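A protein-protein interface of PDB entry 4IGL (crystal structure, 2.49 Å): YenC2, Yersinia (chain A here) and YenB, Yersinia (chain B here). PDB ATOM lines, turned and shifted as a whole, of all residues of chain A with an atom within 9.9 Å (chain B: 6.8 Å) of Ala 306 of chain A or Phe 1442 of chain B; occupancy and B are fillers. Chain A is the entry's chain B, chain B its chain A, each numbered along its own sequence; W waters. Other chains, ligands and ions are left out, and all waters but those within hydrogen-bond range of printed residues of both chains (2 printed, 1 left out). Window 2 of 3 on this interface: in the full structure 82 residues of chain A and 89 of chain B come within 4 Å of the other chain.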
ATOM      1  N   SER A 284       5.457 -21.992  -0.932  1.00  0.00           N
ATOM      2  CA  SER A 284       6.572 -21.131  -0.552  1.00  0.00           C
ATOM      3  C   SER A 284       6.478 -20.824   0.936  1.00  0.00           C
ATOM      4  O   SER A 284       5.495 -21.180   1.589  1.00  0.00           O
ATOM      5  CB  SER A 284       6.552 -19.828  -1.351  1.00  0.00           C
ATOM      6  OG  SER A 284       5.458 -19.017  -0.970  1.00  0.00           O
ATOM      7  N   ALA A 285       7.492 -20.159   1.475  1.00  0.00           N
ATOM      8  CA  ALA A 285       7.462 -19.790   2.883  1.00  0.00           C
ATOM      9  C   ALA A 285       6.284 -18.863   3.168  1.00  0.00           C
ATOM     10  O   ALA A 285       5.760 -18.836   4.282  1.00  0.00           O
ATOM     11  CB  ALA A 285       8.775 -19.138   3.291  1.00  0.00           C
ATOM     12  N   ALA A 286       5.856 -18.128   2.144  1.00  0.00           N
ATOM     13  CA  ALA A 286       4.728 -17.210   2.269  1.00  0.00           C
ATOM     14  C   ALA A 286       3.381 -17.899   2.056  1.00  0.00           C
ATOM     15  O   ALA A 286       2.337 -17.245   2.035  1.00  0.00           O
ATOM     16  CB  ALA A 286       4.886 -16.060   1.289  1.00  0.00           C
ATOM     17  N   GLN A 288       2.387 -19.475  -0.635  1.00  0.00           N
ATOM     18  CA  GLN A 288       1.945 -19.480  -2.025  1.00  0.00           C
ATOM     19  C   GLN A 288       2.309 -20.828  -2.640  1.00  0.00           C
ATOM     20  O   GLN A 288       3.373 -21.382  -2.343  1.00  0.00           O
ATOM     21  CB  GLN A 288       2.640 -18.377  -2.820  1.00  0.00           C
ATOM     22  CG  GLN A 288       2.657 -17.016  -2.160  1.00  0.00           C
ATOM     23  CD  GLN A 288       3.881 -16.213  -2.579  1.00  0.00           C
ATOM     24  OE1 GLN A 288       5.016 -16.707  -2.509  1.00  0.00           O
ATOM     25  NE2 GLN A 288       3.662 -14.973  -3.015  1.00  0.00           N
ATOM     26  N   THR A 303       7.417 -19.552  -9.827  1.00  0.00           N
ATOM     27  CA  THR A 303       8.625 -18.836  -9.448  1.00  0.00           C
ATOM     28  C   THR A 303       8.272 -17.454  -8.927  1.00  0.00           C
ATOM     29  O   THR A 303       7.520 -16.710  -9.569  1.00  0.00           O
ATOM     30  CB  THR A 303       9.578 -18.681 -10.645  1.00  0.00           C
ATOM     31  OG1 THR A 303       9.656 -19.924 -11.355  1.00  0.00           O
ATOM     32  CG2 THR A 303      10.968 -18.278 -10.173  1.00  0.00           C
ATOM     33  N   TYR A 304       8.834 -17.111  -7.770  1.00  0.00           N
ATOM     34  CA  TYR A 304       8.539 -15.837  -7.122  1.00  0.00           C
ATOM     35  C   TYR A 304       9.778 -14.970  -6.950  1.00  0.00           C
ATOM     36  O   TYR A 304      10.901 -15.472  -6.869  1.00  0.00           O
ATOM     37  CB  TYR A 304       7.877 -16.069  -5.764  1.00  0.00           C
ATOM     38  CG  TYR A 304       6.567 -16.818  -5.851  1.00  0.00           C
ATOM     39  CD1 TYR A 304       5.369 -16.137  -6.016  1.00  0.00           C
ATOM     40  CD2 TYR A 304       6.530 -18.204  -5.773  1.00  0.00           C
ATOM     41  CE1 TYR A 304       4.169 -16.817  -6.097  1.00  0.00           C
ATOM     42  CE2 TYR A 304       5.340 -18.893  -5.851  1.00  0.00           C
ATOM     43  CZ  TYR A 304       4.161 -18.198  -6.015  1.00  0.00           C
ATOM     44  OH  TYR A 304       2.973 -18.892  -6.092  1.00  0.00           O
ATOM     45  N   GLU A 305       9.555 -13.661  -6.897  1.00  0.00           N
ATOM     46  CA  GLU A 305      10.617 -12.698  -6.655  1.00  0.00           C
ATOM     47  C   GLU A 305      10.858 -12.607  -5.154  1.00  0.00           C
ATOM     48  O   GLU A 305       9.935 -12.333  -4.388  1.00  0.00           O
ATOM     49  CB  GLU A 305      10.226 -11.330  -7.223  1.00  0.00           C
ATOM     50  CG  GLU A 305      11.348 -10.300  -7.244  1.00  0.00           C
ATOM     51  CD  GLU A 305      10.912  -8.973  -7.848  1.00  0.00           C
ATOM     52  OE1 GLU A 305       9.778  -8.524  -7.569  1.00  0.00           O
ATOM     53  OE2 GLU A 305      11.709  -8.381  -8.607  1.00  0.00           O
ATOM     54  N   ALA A 306      12.098 -12.845  -4.741  1.00  0.00           N
ATOM     55  CA  ALA A 306      12.447 -12.949  -3.324  1.00  0.00           C
ATOM     56  C   ALA A 306      12.143 -11.695  -2.511  1.00  0.00           C
ATOM     57  O   ALA A 306      11.679 -11.780  -1.372  1.00  0.00           O
ATOM     58  CB  ALA A 306      13.913 -13.324  -3.175  1.00  0.00           C
ATOM     59  N   GLU A 307      12.397 -10.532  -3.100  1.00  0.00           N
ATOM     60  CA  GLU A 307      12.202  -9.267  -2.403  1.00  0.00           C
ATOM     61  C   GLU A 307      10.729  -8.931  -2.210  1.00  0.00           C
ATOM     62  O   GLU A 307      10.347  -8.342  -1.198  1.00  0.00           O
ATOM     63  CB  GLU A 307      12.885  -8.125  -3.163  1.00  0.00           C
ATOM     64  CG  GLU A 307      14.402  -8.239  -3.258  1.00  0.00           C
ATOM     65  CD  GLU A 307      14.866  -9.070  -4.441  1.00  0.00           C
ATOM     66  OE1 GLU A 307      14.091  -9.928  -4.919  1.00  0.00           O
ATOM     67  OE2 GLU A 307      16.014  -8.864  -4.894  1.00  0.00           O
ATOM     68  N   THR A 308       9.905  -9.319  -3.181  1.00  0.00           N
ATOM     69  CA  THR A 308       8.529  -8.839  -3.245  1.00  0.00           C
ATOM     70  C   THR A 308       7.453  -9.915  -3.122  1.00  0.00           C
ATOM     71  O   THR A 308       6.274  -9.593  -2.980  1.00  0.00           O
ATOM     72  CB  THR A 308       8.288  -8.100  -4.573  1.00  0.00           C
ATOM     73  OG1 THR A 308       8.575  -8.981  -5.667  1.00  0.00           O
ATOM     74  CG2 THR A 308       9.171  -6.859  -4.663  1.00  0.00           C
ATOM     75  N   GLN A 309       7.854 -11.181  -3.195  1.00  0.00           N
ATOM     76  CA  GLN A 309       6.904 -12.293  -3.304  1.00  0.00           C
ATOM     77  C   GLN A 309       5.977 -12.181  -4.515  1.00  0.00           C
ATOM     78  O   GLN A 309       4.876 -12.737  -4.518  1.00  0.00           O
ATOM     79  CB  GLN A 309       6.090 -12.490  -2.017  1.00  0.00           C
ATOM     80  CG  GLN A 309       6.824 -13.274  -0.943  1.00  0.00           C
ATOM     81  CD  GLN A 309       7.562 -14.479  -1.508  1.00  0.00           C
ATOM     82  OE1 GLN A 309       8.772 -14.423  -1.749  1.00  0.00           O
ATOM     83  NE2 GLN A 309       6.839 -15.578  -1.720  1.00  0.00           N
ATOM     84  N   ARG A 310       6.429 -11.474  -5.547  1.00  0.00           N
ATOM     85  CA  ARG A 310       5.656 -11.368  -6.777  1.00  0.00           C
ATOM     86  C   ARG A 310       5.866 -12.598  -7.653  1.00  0.00           C
ATOM     87  O   ARG A 310       6.972 -13.132  -7.742  1.00  0.00           O
ATOM     88  CB  ARG A 310       6.028 -10.102  -7.555  1.00  0.00           C
ATOM     89  CG  ARG A 310       5.581  -8.800  -6.907  1.00  0.00           C
ATOM     90  CD  ARG A 310       6.068  -7.606  -7.709  1.00  0.00           C
ATOM     91  NE  ARG A 310       5.942  -6.352  -6.971  1.00  0.00           N
ATOM     92  CZ  ARG A 310       6.392  -5.183  -7.410  1.00  0.00           C
ATOM     93  NH1 ARG A 310       6.994  -5.104  -8.587  1.00  0.00           N
ATOM     94  NH2 ARG A 310       6.242  -4.091  -6.671  1.00  0.00           N
ATOM     95  N   LEU A 311       4.790 -13.040  -8.294  1.00  0.00           N
ATOM     96  CA  LEU A 311       4.838 -14.179  -9.197  1.00  0.00           C
ATOM     97  C   LEU A 311       5.460 -13.776 -10.531  1.00  0.00           C
ATOM     98  O   LEU A 311       4.832 -13.074 -11.327  1.00  0.00           O
ATOM     99  CB  LEU A 311       3.425 -14.723  -9.423  1.00  0.00           C
ATOM    100  CG  LEU A 311       3.325 -15.995 -10.267  1.00  0.00           C
ATOM    101  CD1 LEU A 311       4.234 -17.074  -9.702  1.00  0.00           C
ATOM    102  CD2 LEU A 311       1.888 -16.494 -10.342  1.00  0.00           C
ATOM    103  N   ILE A 312       6.688 -14.224 -10.777  1.00  0.00           N
ATOM    104  CA  ILE A 312       7.387 -13.880 -12.016  1.00  0.00           C
ATOM    105  C   ILE A 312       7.527 -15.077 -12.949  1.00  0.00           C
ATOM    106  O   ILE A 312       7.993 -14.935 -14.084  1.00  0.00           O
ATOM    107  CB  ILE A 312       8.798 -13.300 -11.745  1.00  0.00           C
ATOM    108  CG1 ILE A 312       9.757 -14.408 -11.291  1.00  0.00           C
ATOM    109  CG2 ILE A 312       8.725 -12.160 -10.733  1.00  0.00           C
ATOM    110  CD1 ILE A 312      11.175 -13.936 -11.035  1.00  0.00           C
ATOM    111  N   GLY A 313       7.120 -16.252 -12.478  1.00  0.00           N
ATOM    112  CA  GLY A 313       7.192 -17.442 -13.312  1.00  0.00           C
ATOM    113  C   GLY A 313       6.044 -18.414 -13.124  1.00  0.00           C
ATOM    114  O   GLY A 313       5.681 -18.744 -12.000  1.00  0.00           O
ATOM    115  N   TRP B1378      17.337 -22.527   4.771  1.00  0.00           N
ATOM    116  CA  TRP B1378      18.642 -22.139   5.287  1.00  0.00           C
ATOM    117  C   TRP B1378      18.921 -22.870   6.586  1.00  0.00           C
ATOM    118  O   TRP B1378      18.036 -23.478   7.186  1.00  0.00           O
ATOM    119  CB  TRP B1378      18.771 -20.632   5.517  1.00  0.00           C
ATOM    120  CG  TRP B1378      18.911 -19.856   4.254  1.00  0.00           C
ATOM    121  CD1 TRP B1378      20.012 -19.809   3.447  1.00  0.00           C
ATOM    122  CD2 TRP B1378      17.990 -18.899   3.724  1.00  0.00           C
ATOM    123  NE1 TRP B1378      19.797 -18.950   2.399  1.00  0.00           N
ATOM    124  CE2 TRP B1378      18.566 -18.367   2.551  1.00  0.00           C
ATOM    125  CE3 TRP B1378      16.718 -18.463   4.108  1.00  0.00           C
ATOM    126  CZ2 TRP B1378      17.914 -17.424   1.759  1.00  0.00           C
ATOM    127  CZ3 TRP B1378      16.069 -17.528   3.318  1.00  0.00           C
ATOM    128  CH2 TRP B1378      16.670 -17.017   2.157  1.00  0.00           C
ATOM    129  N   VAL B1420      10.370  -5.053   8.392  1.00  0.00           N
ATOM    130  CA  VAL B1420       9.423  -6.151   8.236  1.00  0.00           C
ATOM    131  C   VAL B1420       9.970  -7.121   7.188  1.00  0.00           C
ATOM    132  O   VAL B1420      10.192  -6.756   6.029  1.00  0.00           O
ATOM    133  CB  VAL B1420       7.975  -5.673   7.913  1.00  0.00           C
ATOM    134  CG1 VAL B1420       7.949  -4.778   6.691  1.00  0.00           C
ATOM    135  CG2 VAL B1420       7.052  -6.866   7.718  1.00  0.00           C
ATOM    136  N   TYR B1421      10.242  -8.345   7.627  1.00  0.00           N
ATOM    137  CA  TYR B1421      10.940  -9.325   6.800  1.00  0.00           C
ATOM    138  C   TYR B1421       9.992 -10.166   5.954  1.00  0.00           C
ATOM    139  O   TYR B1421       8.873 -10.477   6.372  1.00  0.00           O
ATOM    140  CB  TYR B1421      11.793 -10.247   7.675  1.00  0.00           C
ATOM    141  CG  TYR B1421      13.063  -9.623   8.208  1.00  0.00           C
ATOM    142  CD1 TYR B1421      14.258  -9.735   7.510  1.00  0.00           C
ATOM    143  CD2 TYR B1421      13.073  -8.938   9.415  1.00  0.00           C
ATOM    144  CE1 TYR B1421      15.423  -9.174   7.990  1.00  0.00           C
ATOM    145  CE2 TYR B1421      14.233  -8.379   9.907  1.00  0.00           C
ATOM    146  CZ  TYR B1421      15.404  -8.501   9.190  1.00  0.00           C
ATOM    147  OH  TYR B1421      16.562  -7.943   9.673  1.00  0.00           O
ATOM    148  N   GLN B1422      10.454 -10.544   4.766  1.00  0.00           N
ATOM    149  CA  GLN B1422       9.737 -11.518   3.959  1.00  0.00           C
ATOM    150  C   GLN B1422       9.814 -12.852   4.688  1.00  0.00           C
ATOM    151  O   GLN B1422      10.786 -13.118   5.393  1.00  0.00           O
ATOM    152  CB  GLN B1422      10.374 -11.641   2.568  1.00  0.00           C
ATOM    153  CG  GLN B1422      10.145 -10.432   1.672  1.00  0.00           C
ATOM    154  CD  GLN B1422       8.699 -10.299   1.204  1.00  0.00           C
ATOM    155  OE1 GLN B1422       7.897 -11.226   1.342  1.00  0.00           O
ATOM    156  NE2 GLN B1422       8.358  -9.133   0.664  1.00  0.00           N
ATOM    157  N   PRO B1423       8.783 -13.691   4.533  1.00  0.00           N
ATOM    158  CA  PRO B1423       8.797 -15.046   5.098  1.00  0.00           C
ATOM    159  C   PRO B1423      10.012 -15.850   4.625  1.00  0.00           C
ATOM    160  O   PRO B1423      10.508 -15.607   3.524  1.00  0.00           O
ATOM    161  CB  PRO B1423       7.507 -15.660   4.548  1.00  0.00           C
ATOM    162  CG  PRO B1423       6.600 -14.486   4.335  1.00  0.00           C
ATOM    163  CD  PRO B1423       7.498 -13.372   3.882  1.00  0.00           C
ATOM    164  N   TYR B1424      10.490 -16.781   5.448  1.00  0.00           N
ATOM    165  CA  TYR B1424      11.640 -17.608   5.082  1.00  0.00           C
ATOM    166  C   TYR B1424      11.630 -18.995   5.731  1.00  0.00           C
ATOM    167  O   TYR B1424      11.060 -19.185   6.804  1.00  0.00           O
ATOM    168  CB  TYR B1424      12.950 -16.878   5.395  1.00  0.00           C
ATOM    169  CG  TYR B1424      13.146 -16.526   6.860  1.00  0.00           C
ATOM    170  CD1 TYR B1424      13.767 -17.410   7.738  1.00  0.00           C
ATOM    171  CD2 TYR B1424      12.720 -15.301   7.358  1.00  0.00           C
ATOM    172  CE1 TYR B1424      13.953 -17.085   9.072  1.00  0.00           C
ATOM    173  CE2 TYR B1424      12.895 -14.968   8.684  1.00  0.00           C
ATOM    174  CZ  TYR B1424      13.516 -15.860   9.538  1.00  0.00           C
ATOM    175  OH  TYR B1424      13.692 -15.526  10.865  1.00  0.00           O
ATOM    176  N   ALA B1437      19.978 -11.951   9.879  1.00  0.00           N
ATOM    177  CA  ALA B1437      18.750 -11.576   9.181  1.00  0.00           C
ATOM    178  C   ALA B1437      18.923 -10.305   8.355  1.00  0.00           C
ATOM    179  O   ALA B1437      18.511 -10.242   7.192  1.00  0.00           O
ATOM    180  CB  ALA B1437      17.611 -11.407  10.182  1.00  0.00           C
ATOM    181  N   ARG B1438      19.539  -9.299   8.966  1.00  0.00           N
ATOM    182  CA  ARG B1438      19.800  -8.025   8.315  1.00  0.00           C
ATOM    183  C   ARG B1438      20.775  -8.228   7.174  1.00  0.00           C
ATOM    184  O   ARG B1438      20.693  -7.551   6.150  1.00  0.00           O
ATOM    185  CB  ARG B1438      20.390  -7.012   9.299  1.00  0.00           C
ATOM    186  CG  ARG B1438      19.452  -6.540  10.402  1.00  0.00           C
ATOM    187  CD  ARG B1438      20.124  -5.465  11.244  1.00  0.00           C
ATOM    188  NE  ARG B1438      19.424  -5.220  12.506  1.00  0.00           N
ATOM    189  CZ  ARG B1438      19.890  -5.588  13.697  1.00  0.00           C
ATOM    190  NH1 ARG B1438      21.055  -6.217  13.783  1.00  0.00           N
ATOM    191  NH2 ARG B1438      19.195  -5.332  14.800  1.00  0.00           N
ATOM    192  N   ASP B1440      21.352 -11.190   5.393  1.00  0.00           N
ATOM    193  CA  ASP B1440      20.980 -12.170   4.373  1.00  0.00           C
ATOM    194  C   ASP B1440      19.483 -12.318   4.066  1.00  0.00           C
ATOM    195  O   ASP B1440      19.112 -13.009   3.117  1.00  0.00           O
ATOM    196  CB  ASP B1440      21.573 -13.537   4.731  1.00  0.00           C
ATOM    197  CG  ASP B1440      23.095 -13.541   4.709  1.00  0.00           C
ATOM    198  OD1 ASP B1440      23.672 -13.210   3.650  1.00  0.00           O
ATOM    199  OD2 ASP B1440      23.712 -13.870   5.750  1.00  0.00           O
ATOM    200  N   LEU B1441      18.619 -11.674   4.840  1.00  0.00           N
ATOM    201  CA  LEU B1441      17.186 -11.822   4.592  1.00  0.00           C
ATOM    202  C   LEU B1441      16.573 -10.534   4.054  1.00  0.00           C
ATOM    203  O   LEU B1441      16.993  -9.438   4.412  1.00  0.00           O
ATOM    204  CB  LEU B1441      16.456 -12.294   5.851  1.00  0.00           C
ATOM    205  CG  LEU B1441      16.905 -13.671   6.358  1.00  0.00           C
ATOM    206  CD1 LEU B1441      16.102 -14.122   7.581  1.00  0.00           C
ATOM    207  CD2 LEU B1441      16.829 -14.698   5.245  1.00  0.00           C
ATOM    208  N   PHE B1442      15.593 -10.675   3.171  1.00  0.00           N
ATOM    209  CA  PHE B1442      14.939  -9.516   2.575  1.00  0.00           C
ATOM    210  C   PHE B1442      13.900  -8.888   3.497  1.00  0.00           C
ATOM    211  O   PHE B1442      13.088  -9.583   4.111  1.00  0.00           O
ATOM    212  CB  PHE B1442      14.311  -9.878   1.227  1.00  0.00           C
ATOM    213  CG  PHE B1442      15.319 -10.079   0.129  1.00  0.00           C
ATOM    214  CD1 PHE B1442      16.120  -9.022  -0.294  1.00  0.00           C
ATOM    215  CD2 PHE B1442      15.467 -11.314  -0.483  1.00  0.00           C
ATOM    216  CE1 PHE B1442      17.052  -9.197  -1.305  1.00  0.00           C
ATOM    217  CE2 PHE B1442      16.396 -11.497  -1.496  1.00  0.00           C
ATOM    218  CZ  PHE B1442      17.188 -10.438  -1.909  1.00  0.00           C
ATOM    219  N   ALA B1443      13.935  -7.563   3.585  1.00  0.00           N
ATOM    220  CA  ALA B1443      13.011  -6.835   4.436  1.00  0.00           C
ATOM    221  C   ALA B1443      12.719  -5.471   3.851  1.00  0.00           C
ATOM    222  O   ALA B1443      13.538  -4.897   3.135  1.00  0.00           O
ATOM    223  CB  ALA B1443      13.589  -6.687   5.837  1.00  0.00           C
ATOM    224  N   ASP B1444      11.535  -4.960   4.142  1.00  0.00           N
ATOM    225  CA  ASP B1444      11.255  -3.568   3.867  1.00  0.00           C
ATOM    226  C   ASP B1444      11.563  -2.803   5.146  1.00  0.00           C
ATOM    227  O   ASP B1444      11.203  -3.243   6.240  1.00  0.00           O
ATOM    228  CB  ASP B1444       9.797  -3.376   3.440  1.00  0.00           C
ATOM    229  CG  ASP B1444       9.485  -4.036   2.099  1.00  0.00           C
ATOM    230  OD1 ASP B1444      10.435  -4.357   1.351  1.00  0.00           O
ATOM    231  OD2 ASP B1444       8.289  -4.230   1.794  1.00  0.00           O
ATOM    232  N   ALA B1460      12.884  -3.958  -0.160  1.00  0.00           N
ATOM    233  CA  ALA B1460      14.018  -4.871  -0.253  1.00  0.00           C
ATOM    234  C   ALA B1460      14.755  -4.680  -1.572  1.00  0.00           C
ATOM    235  O   ALA B1460      15.985  -4.700  -1.616  1.00  0.00           O
ATOM    236  CB  ALA B1460      13.553  -6.307  -0.102  1.00  0.00           C
ATOM    237  N   LYS B1461      13.984  -4.484  -2.640  1.00  0.00           N
ATOM    238  CA  LYS B1461      14.522  -4.247  -3.979  1.00  0.00           C
ATOM    239  C   LYS B1461      15.299  -2.934  -4.051  1.00  0.00           C
ATOM    240  O   LYS B1461      16.144  -2.752  -4.927  1.00  0.00           O
ATOM    241  CB  LYS B1461      13.383  -4.238  -5.008  1.00  0.00           C
ATOM    242  CG  LYS B1461      13.364  -5.404  -6.000  1.00  0.00           C
ATOM    243  CD  LYS B1461      14.071  -5.041  -7.299  1.00  0.00           C
ATOM    244  CE  LYS B1461      13.795  -6.054  -8.404  1.00  0.00           C
ATOM    245  NZ  LYS B1461      12.358  -6.104  -8.799  1.00  0.00           N
HETATM  246  O   HOH W   1      10.410  -7.206   1.845  1.00  0.00           O
HETATM  247  O   HOH W   2       9.173  -6.695  -9.495  1.00  0.00           O
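Of chain B, only Gln 1422 (3.7 Å) and Phe 1442 (3.5 Å) come within 4 Å of Ala 306 of chain A. Of chain A, only Ala 306 (3.5 Å) and Glu 307 (3.4 Å) come within 4 Å of Phe 1442 of chain B. Gln 1422 of chain B touches just these residues of chain A: Ala 306 (3.7 Å), Glu 307 (2.8 Å), Thr 308 (3.9 Å) and Gln 309 (3.3 Å). Ala 1443 of chain B touches none of the printed residues of chain A. Printed residues of chain B within 4 Å of Thr 308 of chain A: Gln 1422 (3.9 Å). Printed residues of chain A within 4 Å of Pro 1423 of chain B: Ala 285 and Ala 286. Of the printed residues of chain B, Glu 305 of chain A touches Lys 1461 (2.4 Å). Of the printed residues of chain B, Ala 286 of chain A touches Pro 1423. Printed residues of chain A within 4 Å of Lys 1461 of chain B: Glu 305 and Glu 307. Gly 313 of chain A touches none of the printed residues of chain B. The nearest printed residue of chain A that does not touch Pro 1423 of chain B is Gln 309 of chain A (4.9 Å).
The backbone NH (N) of Gln 1422 of chain B lies within hydrogen-bond range of the backbone carbonyl oxygen (O) of Phe 1442 of chain B, 2.9 Å away. The backbone NH (N) of Ala 1460 of chain B sits close to the backbone carbonyl oxygen (O) of Ala 1443 of chain B (3.5 Å). OD1 of Asp 1444 of chain B lies within hydrogen-bond range of N of Ala 1460 of chain B (2.9 Å). OG of Ser 284 of chain A sits close to N of Ala 286 of chain A (3.3 Å). The backbone carbonyl oxygen (O) of Gln 309 of chain A lies within hydrogen-bond range of the side-chain amide nitrogen (NE2) of Gln 288 of chain A, 3.0 Å away. The backbone carbonyl oxygen of Arg 310 of chain A sits at hydrogen-bond distance from the backbone NH of Glu 305 of chain A (2.8 Å).
Water W2 lies within hydrogen-bond range of OE1 of Glu 305 of chain A (2.7 Å), NH1 of Arg 310 of chain A (2.8 Å) and NZ of Lys 1461 of chain B (3.3 Å). Water W1 lies within hydrogen-bond range of the side-chain carboxylate of Asp 1444 of chain B (2.9 Å), the side-chain amide nitrogen of Gln 1422 of chain B (3.1 Å) and the backbone carbonyl oxygen of Glu 307 of chain A (3.2 Å).
Of the 15 printed residues of chain A, 7 touch a printed residue of chain B. Printed residues of chain A that touch a printed residue of chain B: Ala 285, Ala 286, Glu 305, Ala 306, Glu 307, Thr 308 and Gln 309. Along chain A the printed residues that touch a printed residue of chain B span positions 285 to 309. Of the 15 printed residues of chain B, 6 touch a printed residue of chain A. Printed residues of chain B that touch a printed residue of chain A: Gln 1422, Pro 1423, Tyr 1424, Phe 1442, Ala 1460 and Lys 1461. Hydrophobic or aromatic side chains of chain B within 4 Å of the printed part of chain A: Pro 1423, Phe 1442 and Ala 1460. Among the printed residues, 12 pairs touch across the chains.
Among the printed residues, merely in contact across the chains: Ala 285 of chain A with Pro 1423 of chain B, Ala 285 of chain A with Tyr 1424 of chain B, Ala 286 of chain A with Pro 1423 of chain B, Ala 306 of chain A with Gln 1422 of chain B, Ala 306 of chain A with Phe 1442 of chain B, Glu 307 of chain A with Phe 1442 of chain B, Glu 307 of chain A with Ala 1460 of chain B, Glu 307 of chain A with Lys 1461 of chain B, Thr 308 of chain A with Gln 1422 of chain B and Gln 309 of chain A with Gln 1422 of chain B.
The side-chain amide nitrogen of Gln 1422 of chain B lies within hydrogen-bond range of the backbone carbonyl oxygen of Glu 307 of chain A (2.8 Å). The side-chain carboxylate of Glu 305 of chain A lies within salt-bridge range of the side-chain amino group of Lys 1461 of chain B, 3.7 Å away.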
